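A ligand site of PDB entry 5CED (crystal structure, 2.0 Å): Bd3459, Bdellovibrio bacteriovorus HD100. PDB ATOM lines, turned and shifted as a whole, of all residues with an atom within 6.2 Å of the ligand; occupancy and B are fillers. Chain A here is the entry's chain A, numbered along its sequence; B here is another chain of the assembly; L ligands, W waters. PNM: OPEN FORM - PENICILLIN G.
Water W1 bridges an oxygen (O12) of the ligand (2.6 Å) and the side-chain amino group (NZ) of Lys 365 (2.9 Å).
The side-chain hydroxyl (OG) of Ser 290 lies within hydrogen-bond range of the backbone NH (N) of Asn 292 (3.1 Å).
The backbone carbonyl oxygen of Gly 359 lies within hydrogen-bond range of the backbone NH of Thr 366.
The side-chain amino group of Lys 365 lies within hydrogen-bond range of the backbone carbonyl oxygen of Gly 359 (3.2 Å).
The side-chain amino group of Lys 365 is in hydrogen-bond range of the side-chain hydroxyl of Ser 360, at 2.8 Å.
OE1 of Glu 38 of chain B sits at hydrogen-bond distance from OH of Tyr 388 (2.6 Å).
O of Val 361 sits at hydrogen-bond distance from NE1 of Trp 395, at 2.9 Å.
OG1 of Thr 358 is in hydrogen-bond range of NZ of Lys 357.
OG1 of Thr 358 is in hydrogen-bond range of OG1 of Thr 342 (2.6 Å).
CB of Ala 69 touches O8 of the ligand, at 3.4 Å.
Gln 250 touches the ligand (NE2 to C9, 3.6 Å).
CG2 of Thr 342 touches O13 of the ligand (3.6 Å).
CA of Gly 359 touches O8 of the ligand, at 3.3 Å.
Trp 395 touches the ligand (CH2 to C23, 3.9 Å).
Glu 38 of chain B touches the ligand (OE2 to C21, 3.5 Å).
Hydrophobic or aromatic side chains that line the ligand: Ala 69 and Trp 395.
Of the 25 residues printed, 12 come within 4 Å of the ligand.
Along chain A the residues within 4 Å of the ligand span positions 69 to 395.
The nearest printed residue that does not touch the ligand is Ser 251 (4.1 Å).
An oxygen (O13) of the ligand sits at hydrogen-bond distance from the side-chain hydroxyl (OG1) of Thr 358, at 2.6 Å.
C7 of the ligand is bonded to OG of Ser 70 (1.4 Å).
O16 of the ligand lies within hydrogen-bond range of ND2 of Asn 292.
An oxygen (O8) of the ligand sits close to the backbone NH of Ser 70, at 2.8 Å.
An oxygen (O8) of the ligand lies within hydrogen-bond range of the backbone NH (N) of Ser 360 (2.9 Å).
An oxygen (O12) of the ligand lies within salt-bridge range of the side-chain amino group (NZ) of Lys 365 (3.6 Å).
The side-chain hydroxyl of Ser 360 sits at hydrogen-bond distance from an oxygen (O12) of the ligand (2.7 Å).
An oxygen (O13) of the ligand is in salt-bridge range of the side-chain amino group (NZ) of Lys 357 (3.5 Å).
The backbone carbonyl oxygen of Ser 360 lies within hydrogen-bond range of a nitrogen (N14) of the ligand (3.0 Å).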
ATOM      1  N   LEU A  68     -27.686  37.501  30.858  1.00  0.00           N
ATOM      2  CA  LEU A  68     -27.447  37.547  29.423  1.00  0.00           C
ATOM      3  C   LEU A  68     -27.441  36.194  28.702  1.00  0.00           C
ATOM      4  O   LEU A  68     -27.747  36.142  27.504  1.00  0.00           O
ATOM      5  CB  LEU A  68     -26.130  38.258  29.171  1.00  0.00           C
ATOM      6  CG  LEU A  68     -26.016  39.696  29.645  1.00  0.00           C
ATOM      7  CD1 LEU A  68     -24.634  40.177  29.182  1.00  0.00           C
ATOM      8  CD2 LEU A  68     -27.104  40.603  29.102  1.00  0.00           C
ATOM      9  N   ALA A  69     -27.087  35.125  29.435  1.00  0.00           N
ATOM     10  CA  ALA A  69     -26.741  33.839  28.881  1.00  0.00           C
ATOM     11  C   ALA A  69     -25.692  34.004  27.752  1.00  0.00           C
ATOM     12  O   ALA A  69     -24.808  34.897  27.840  1.00  0.00           O
ATOM     13  CB  ALA A  69     -28.023  33.118  28.372  1.00  0.00           C
ATOM     14  N   SER A  70     -25.785  33.384  26.619  1.00  0.00           N
ATOM     15  CA  SER A  70     -24.720  33.235  25.679  1.00  0.00           C
ATOM     16  C   SER A  70     -24.594  34.431  24.704  1.00  0.00           C
ATOM     17  O   SER A  70     -23.556  34.485  24.019  1.00  0.00           O
ATOM     18  CB  SER A  70     -24.874  32.026  24.761  1.00  0.00           C
ATOM     19  OG  SER A  70     -24.543  30.881  25.530  1.00  0.00           O
ATOM     20  N   ILE A  71     -25.340  35.502  24.994  1.00  0.00           N
ATOM     21  CA  ILE A  71     -25.035  36.766  24.265  1.00  0.00           C
ATOM     22  C   ILE A  71     -23.812  37.404  24.887  1.00  0.00           C
ATOM     23  O   ILE A  71     -23.202  38.277  24.289  1.00  0.00           O
ATOM     24  CB  ILE A  71     -26.226  37.735  24.113  1.00  0.00           C
ATOM     25  CG1 ILE A  71     -26.682  38.319  25.456  1.00  0.00           C
ATOM     26  CG2 ILE A  71     -27.360  37.055  23.330  1.00  0.00           C
ATOM     27  CD1 ILE A  71     -27.748  39.378  25.333  1.00  0.00           C
ATOM     28  N   LYS A  73     -21.179  35.972  24.837  1.00  0.00           N
ATOM     29  CA  LYS A  73     -20.136  35.669  23.865  1.00  0.00           C
ATOM     30  C   LYS A  73     -19.855  36.816  22.900  1.00  0.00           C
ATOM     31  O   LYS A  73     -18.732  36.921  22.399  1.00  0.00           O
ATOM     32  CB  LYS A  73     -20.424  34.358  23.146  1.00  0.00           C
ATOM     33  CG  LYS A  73     -20.448  33.164  24.083  1.00  0.00           C
ATOM     34  CD  LYS A  73     -20.912  31.874  23.426  1.00  0.00           C
ATOM     35  CE  LYS A  73     -21.001  30.791  24.521  1.00  0.00           C
ATOM     36  NZ  LYS A  73     -21.282  29.445  23.985  1.00  0.00           N
ATOM     37  N   GLN A 250     -22.639  28.425  17.284  1.00  0.00           N
ATOM     38  CA  GLN A 250     -23.135  27.711  18.465  1.00  0.00           C
ATOM     39  C   GLN A 250     -21.914  27.058  19.093  1.00  0.00           C
ATOM     40  O   GLN A 250     -21.142  26.465  18.363  1.00  0.00           O
ATOM     41  CB  GLN A 250     -24.108  26.607  18.069  1.00  0.00           C
ATOM     42  CG  GLN A 250     -24.555  25.672  19.168  1.00  0.00           C
ATOM     43  CD  GLN A 250     -25.752  24.823  18.734  1.00  0.00           C
ATOM     44  OE1 GLN A 250     -25.969  24.574  17.528  1.00  0.00           O
ATOM     45  NE2 GLN A 250     -26.552  24.369  19.713  1.00  0.00           N
ATOM     46  N   SER A 251     -21.791  27.107  20.421  1.00  0.00           N
ATOM     47  CA  SER A 251     -20.621  26.527  21.108  1.00  0.00           C
ATOM     48  C   SER A 251     -20.975  26.243  22.531  1.00  0.00           C
ATOM     49  O   SER A 251     -21.870  26.873  23.089  1.00  0.00           O
ATOM     50  CB  SER A 251     -19.392  27.483  21.044  1.00  0.00           C
ATOM     51  OG  SER A 251     -19.727  28.780  21.455  1.00  0.00           O
ATOM     52  N   ASN A 252     -20.280  25.296  23.130  1.00  0.00           N
ATOM     53  CA  ASN A 252     -20.337  25.169  24.566  1.00  0.00           C
ATOM     54  C   ASN A 252     -19.460  26.322  25.111  1.00  0.00           C
ATOM     55  O   ASN A 252     -19.071  27.258  24.384  1.00  0.00           O
ATOM     56  CB  ASN A 252     -19.933  23.763  25.014  1.00  0.00           C
ATOM     57  CG  ASN A 252     -18.489  23.393  24.686  1.00  0.00           C
ATOM     58  OD1 ASN A 252     -17.580  24.231  24.563  1.00  0.00           O
ATOM     59  ND2 ASN A 252     -18.279  22.113  24.587  1.00  0.00           N
ATOM     60  N   ASN A 253     -19.190  26.279  26.400  1.00  0.00           N
ATOM     61  CA  ASN A 253     -18.552  27.402  27.067  1.00  0.00           C
ATOM     62  C   ASN A 253     -17.043  27.564  26.706  1.00  0.00           C
ATOM     63  O   ASN A 253     -16.480  28.637  26.898  1.00  0.00           O
ATOM     64  CB  ASN A 253     -18.720  27.199  28.568  1.00  0.00           C
ATOM     65  CG  ASN A 253     -17.909  26.029  29.060  1.00  0.00           C
ATOM     66  OD1 ASN A 253     -18.235  24.868  28.752  1.00  0.00           O
ATOM     67  ND2 ASN A 253     -16.800  26.310  29.759  1.00  0.00           N
ATOM     68  N   SER A 290     -18.680  33.081  28.613  1.00  0.00           N
ATOM     69  CA  SER A 290     -19.758  32.356  27.966  1.00  0.00           C
ATOM     70  C   SER A 290     -21.166  32.756  28.440  1.00  0.00           C
ATOM     71  O   SER A 290     -22.107  32.553  27.705  1.00  0.00           O
ATOM     72  CB  SER A 290     -19.615  30.881  28.260  1.00  0.00           C
ATOM     73  OG  SER A 290     -19.795  30.618  29.665  1.00  0.00           O
ATOM     74  N   GLY A 291     -21.268  33.309  29.652  1.00  0.00           N
ATOM     75  CA  GLY A 291     -22.540  33.613  30.282  1.00  0.00           C
ATOM     76  C   GLY A 291     -23.197  32.431  31.028  1.00  0.00           C
ATOM     77  O   GLY A 291     -24.308  32.586  31.556  1.00  0.00           O
ATOM     78  N   ASN A 292     -22.510  31.294  31.108  1.00  0.00           N
ATOM     79  CA  ASN A 292     -23.017  30.109  31.781  1.00  0.00           C
ATOM     80  C   ASN A 292     -22.930  30.310  33.310  1.00  0.00           C
ATOM     81  O   ASN A 292     -22.088  31.053  33.812  1.00  0.00           O
ATOM     82  CB  ASN A 292     -22.204  28.870  31.374  1.00  0.00           C
ATOM     83  CG  ASN A 292     -22.485  28.401  29.934  1.00  0.00           C
ATOM     84  OD1 ASN A 292     -22.583  29.190  28.975  1.00  0.00           O
ATOM     85  ND2 ASN A 292     -22.597  27.116  29.779  1.00  0.00           N
ATOM     86  N   THR A 342     -27.350  28.551  15.753  1.00  0.00           N
ATOM     87  CA  THR A 342     -28.641  28.567  16.467  1.00  0.00           C
ATOM     88  C   THR A 342     -29.749  29.345  15.706  1.00  0.00           C
ATOM     89  O   THR A 342     -30.885  29.236  16.071  1.00  0.00           O
ATOM     90  CB  THR A 342     -28.519  29.147  17.871  1.00  0.00           C
ATOM     91  OG1 THR A 342     -28.091  30.504  17.821  1.00  0.00           O
ATOM     92  CG2 THR A 342     -27.523  28.366  18.713  1.00  0.00           C
ATOM     93  N   LYS A 357     -26.993  36.726  17.874  1.00  0.00           N
ATOM     94  CA  LYS A 357     -26.558  35.726  18.823  1.00  0.00           C
ATOM     95  C   LYS A 357     -27.682  35.424  19.795  1.00  0.00           C
ATOM     96  O   LYS A 357     -28.306  36.324  20.290  1.00  0.00           O
ATOM     97  CB  LYS A 357     -25.327  36.211  19.613  1.00  0.00           C
ATOM     98  CG  LYS A 357     -24.821  35.206  20.664  1.00  0.00           C
ATOM     99  CD  LYS A 357     -23.969  34.093  20.031  1.00  0.00           C
ATOM    100  CE  LYS A 357     -23.876  32.877  20.933  1.00  0.00           C
ATOM    101  NZ  LYS A 357     -25.118  32.043  20.824  1.00  0.00           N
ATOM    102  N   THR A 358     -27.899  34.152  20.099  1.00  0.00           N
ATOM    103  CA  THR A 358     -28.947  33.690  21.019  1.00  0.00           C
ATOM    104  C   THR A 358     -28.333  33.394  22.371  1.00  0.00           C
ATOM    105  O   THR A 358     -27.141  33.164  22.477  1.00  0.00           O
ATOM    106  CB  THR A 358     -29.540  32.340  20.526  1.00  0.00           C
ATOM    107  OG1 THR A 358     -28.454  31.456  20.172  1.00  0.00           O
ATOM    108  CG2 THR A 358     -30.463  32.534  19.269  1.00  0.00           C
ATOM    109  N   GLY A 359     -29.184  33.333  23.394  1.00  0.00           N
ATOM    110  CA  GLY A 359     -28.804  32.821  24.686  1.00  0.00           C
ATOM    111  C   GLY A 359     -29.964  32.124  25.385  1.00  0.00           C
ATOM    112  O   GLY A 359     -31.076  32.511  25.236  1.00  0.00           O
ATOM    113  N   SER A 360     -29.644  31.099  26.167  1.00  0.00           N
ATOM    114  CA  SER A 360     -30.615  30.380  26.984  1.00  0.00           C
ATOM    115  C   SER A 360     -29.949  30.010  28.277  1.00  0.00           C
ATOM    116  O   SER A 360     -28.935  29.363  28.266  1.00  0.00           O
ATOM    117  CB  SER A 360     -31.059  29.098  26.291  1.00  0.00           C
ATOM    118  OG  SER A 360     -31.468  29.332  24.945  1.00  0.00           O
ATOM    119  N   VAL A 361     -30.542  30.394  29.398  1.00  0.00           N
ATOM    120  CA  VAL A 361     -30.219  29.818  30.709  1.00  0.00           C
ATOM    121  C   VAL A 361     -31.518  29.692  31.533  1.00  0.00           C
ATOM    122  O   VAL A 361     -32.602  30.111  31.080  1.00  0.00           O
ATOM    123  CB  VAL A 361     -29.181  30.636  31.524  1.00  0.00           C
ATOM    124  CG1 VAL A 361     -27.815  30.557  30.893  1.00  0.00           C
ATOM    125  CG2 VAL A 361     -29.652  32.079  31.772  1.00  0.00           C
ATOM    126  N   ASN A 362     -31.403  29.159  32.730  1.00  0.00           N
ATOM    127  CA  ASN A 362     -32.571  28.866  33.528  1.00  0.00           C
ATOM    128  C   ASN A 362     -33.543  30.059  33.566  1.00  0.00           C
ATOM    129  O   ASN A 362     -34.733  29.949  33.206  1.00  0.00           O
ATOM    130  CB  ASN A 362     -32.141  28.449  34.911  1.00  0.00           C
ATOM    131  CG  ASN A 362     -33.305  28.212  35.835  1.00  0.00           C
ATOM    132  OD1 ASN A 362     -34.449  27.885  35.407  1.00  0.00           O
ATOM    133  ND2 ASN A 362     -33.037  28.379  37.119  1.00  0.00           N
ATOM    134  N   LYS A 365     -34.022  33.923  28.317  1.00  0.00           N
ATOM    135  CA  LYS A 365     -33.870  33.654  26.920  1.00  0.00           C
ATOM    136  C   LYS A 365     -33.547  35.005  26.280  1.00  0.00           C
ATOM    137  O   LYS A 365     -34.222  35.974  26.537  1.00  0.00           O
ATOM    138  CB  LYS A 365     -35.138  33.080  26.272  1.00  0.00           C
ATOM    139  CG  LYS A 365     -34.898  32.454  24.886  1.00  0.00           C
ATOM    140  CD  LYS A 365     -34.483  31.007  24.997  1.00  0.00           C
ATOM    141  CE  LYS A 365     -34.127  30.357  23.681  1.00  0.00           C
ATOM    142  NZ  LYS A 365     -32.861  30.937  23.116  1.00  0.00           N
ATOM    143  N   THR A 366     -32.491  35.046  25.452  1.00  0.00           N
ATOM    144  CA  THR A 366     -31.998  36.335  24.985  1.00  0.00           C
ATOM    145  C   THR A 366     -31.640  36.304  23.510  1.00  0.00           C
ATOM    146  O   THR A 366     -31.360  35.236  22.923  1.00  0.00           O
ATOM    147  CB  THR A 366     -30.776  36.787  25.836  1.00  0.00           C
ATOM    148  OG1 THR A 366     -29.695  35.874  25.677  1.00  0.00           O
ATOM    149  CG2 THR A 366     -31.140  36.914  27.325  1.00  0.00           C
ATOM    150  N   TYR A 388     -37.175  28.146  33.446  1.00  0.00           N
ATOM    151  CA  TYR A 388     -36.964  26.862  32.803  1.00  0.00           C
ATOM    152  C   TYR A 388     -36.923  25.708  33.806  1.00  0.00           C
ATOM    153  O   TYR A 388     -37.435  24.605  33.495  1.00  0.00           O
ATOM    154  CB  TYR A 388     -35.779  26.969  31.862  1.00  0.00           C
ATOM    155  CG  TYR A 388     -34.934  25.731  31.595  1.00  0.00           C
ATOM    156  CD1 TYR A 388     -34.123  25.236  32.582  1.00  0.00           C
ATOM    157  CD2 TYR A 388     -34.845  25.160  30.333  1.00  0.00           C
ATOM    158  CE1 TYR A 388     -33.301  24.161  32.373  1.00  0.00           C
ATOM    159  CE2 TYR A 388     -33.997  24.078  30.093  1.00  0.00           C
ATOM    160  CZ  TYR A 388     -33.226  23.600  31.136  1.00  0.00           C
ATOM    161  OH  TYR A 388     -32.364  22.531  31.037  1.00  0.00           O
ATOM    162  N   TRP A 395     -38.465  28.090  27.373  1.00  0.00           N
ATOM    163  CA  TRP A 395     -37.507  28.501  26.349  1.00  0.00           C
ATOM    164  C   TRP A 395     -38.146  28.606  24.992  1.00  0.00           C
ATOM    165  O   TRP A 395     -37.961  29.603  24.304  1.00  0.00           O
ATOM    166  CB  TRP A 395     -36.293  27.590  26.292  1.00  0.00           C
ATOM    167  CG  TRP A 395     -35.262  27.816  27.362  1.00  0.00           C
ATOM    168  CD1 TRP A 395     -35.341  28.683  28.446  1.00  0.00           C
ATOM    169  CD2 TRP A 395     -34.047  27.089  27.512  1.00  0.00           C
ATOM    170  NE1 TRP A 395     -34.208  28.555  29.214  1.00  0.00           N
ATOM    171  CE2 TRP A 395     -33.403  27.576  28.674  1.00  0.00           C
ATOM    172  CE3 TRP A 395     -33.426  26.054  26.766  1.00  0.00           C
ATOM    173  CZ2 TRP A 395     -32.182  27.056  29.127  1.00  0.00           C
ATOM    174  CZ3 TRP A 395     -32.212  25.541  27.208  1.00  0.00           C
ATOM    175  CH2 TRP A 395     -31.600  26.068  28.406  1.00  0.00           C
ATOM    176  N   GLU B  38     -30.027  16.040  27.816  1.00  0.00           N
ATOM    177  CA  GLU B  38     -30.073  17.442  27.395  1.00  0.00           C
ATOM    178  C   GLU B  38     -28.734  17.977  26.983  1.00  0.00           C
ATOM    179  O   GLU B  38     -28.643  18.681  25.989  1.00  0.00           O
ATOM    180  CB  GLU B  38     -30.640  18.357  28.470  1.00  0.00           C
ATOM    181  CG  GLU B  38     -31.162  19.674  27.866  1.00  0.00           C
ATOM    182  CD  GLU B  38     -31.452  20.711  28.917  1.00  0.00           C
ATOM    183  OE1 GLU B  38     -31.237  20.387  30.118  1.00  0.00           O
ATOM    184  OE2 GLU B  38     -31.859  21.853  28.549  1.00  0.00           O
ATOM    185  N   GLN B  39     -27.697  17.661  27.748  1.00  0.00           N
ATOM    186  CA  GLN B  39     -26.352  18.206  27.461  1.00  0.00           C
ATOM    187  C   GLN B  39     -25.682  17.586  26.260  1.00  0.00           C
ATOM    188  O   GLN B  39     -24.786  18.176  25.680  1.00  0.00           O
ATOM    189  CB  GLN B  39     -25.476  18.063  28.695  1.00  0.00           C
ATOM    190  CG  GLN B  39     -25.976  18.998  29.767  1.00  0.00           C
ATOM    191  CD  GLN B  39     -25.222  18.894  31.067  1.00  0.00           C
ATOM    192  OE1 GLN B  39     -24.142  18.299  31.140  1.00  0.00           O
ATOM    193  NE2 GLN B  39     -25.786  19.496  32.103  1.00  0.00           N
HETATM  194  O8  PNM L   1     -26.719  30.761  26.283  1.00  0.00           O
HETATM  195  C7  PNM L   1     -25.667  30.184  26.062  1.00  0.00           C
HETATM  196  N4  PNM L   1     -26.018  28.850  24.001  1.00  0.00           N
HETATM  197  C3  PNM L   1     -27.747  28.449  23.916  1.00  0.00           C
HETATM  198  C11 PNM L   1     -28.355  29.317  22.935  1.00  0.00           C
HETATM  199  O13 PNM L   1     -27.618  29.883  22.009  1.00  0.00           O
HETATM  200  O12 PNM L   1     -29.604  29.505  23.013  1.00  0.00           O
HETATM  201  C2  PNM L   1     -27.706  27.037  23.764  1.00  0.00           C
HETATM  202  C10 PNM L   1     -29.013  26.451  24.324  1.00  0.00           C
HETATM  203  C9  PNM L   1     -27.624  26.617  22.275  1.00  0.00           C
HETATM  204  S1  PNM L   1     -26.282  26.476  24.694  1.00  0.00           S
HETATM  205  C5  PNM L   1     -25.423  27.976  24.892  1.00  0.00           C
HETATM  206  C6  PNM L   1     -25.838  28.732  26.188  1.00  0.00           C
HETATM  207  N14 PNM L   1     -26.342  28.172  27.343  1.00  0.00           N
HETATM  208  C15 PNM L   1     -26.011  27.052  28.089  1.00  0.00           C
HETATM  209  O16 PNM L   1     -25.042  26.399  27.848  1.00  0.00           O
HETATM  210  C17 PNM L   1     -27.008  26.808  29.250  1.00  0.00           C
HETATM  211  C18 PNM L   1     -27.567  25.401  29.137  1.00  0.00           C
HETATM  212  C19 PNM L   1     -27.696  24.652  30.319  1.00  0.00           C
HETATM  213  C20 PNM L   1     -28.174  23.325  30.239  1.00  0.00           C
HETATM  214  C21 PNM L   1     -28.513  22.785  29.014  1.00  0.00           C
HETATM  215  C22 PNM L   1     -28.390  23.558  27.832  1.00  0.00           C
HETATM  216  C23 PNM L   1     -27.918  24.858  27.919  1.00  0.00           C
HETATM  217  O   HOH W   1     -31.440  29.331  21.130  1.00  0.00           O
HETATM  218  O   HOH W   2     -23.796  29.379  21.866  1.00  0.00           O
HETATM  219  O   HOH W   3     -24.526  31.065  28.608  1.00  0.00           O
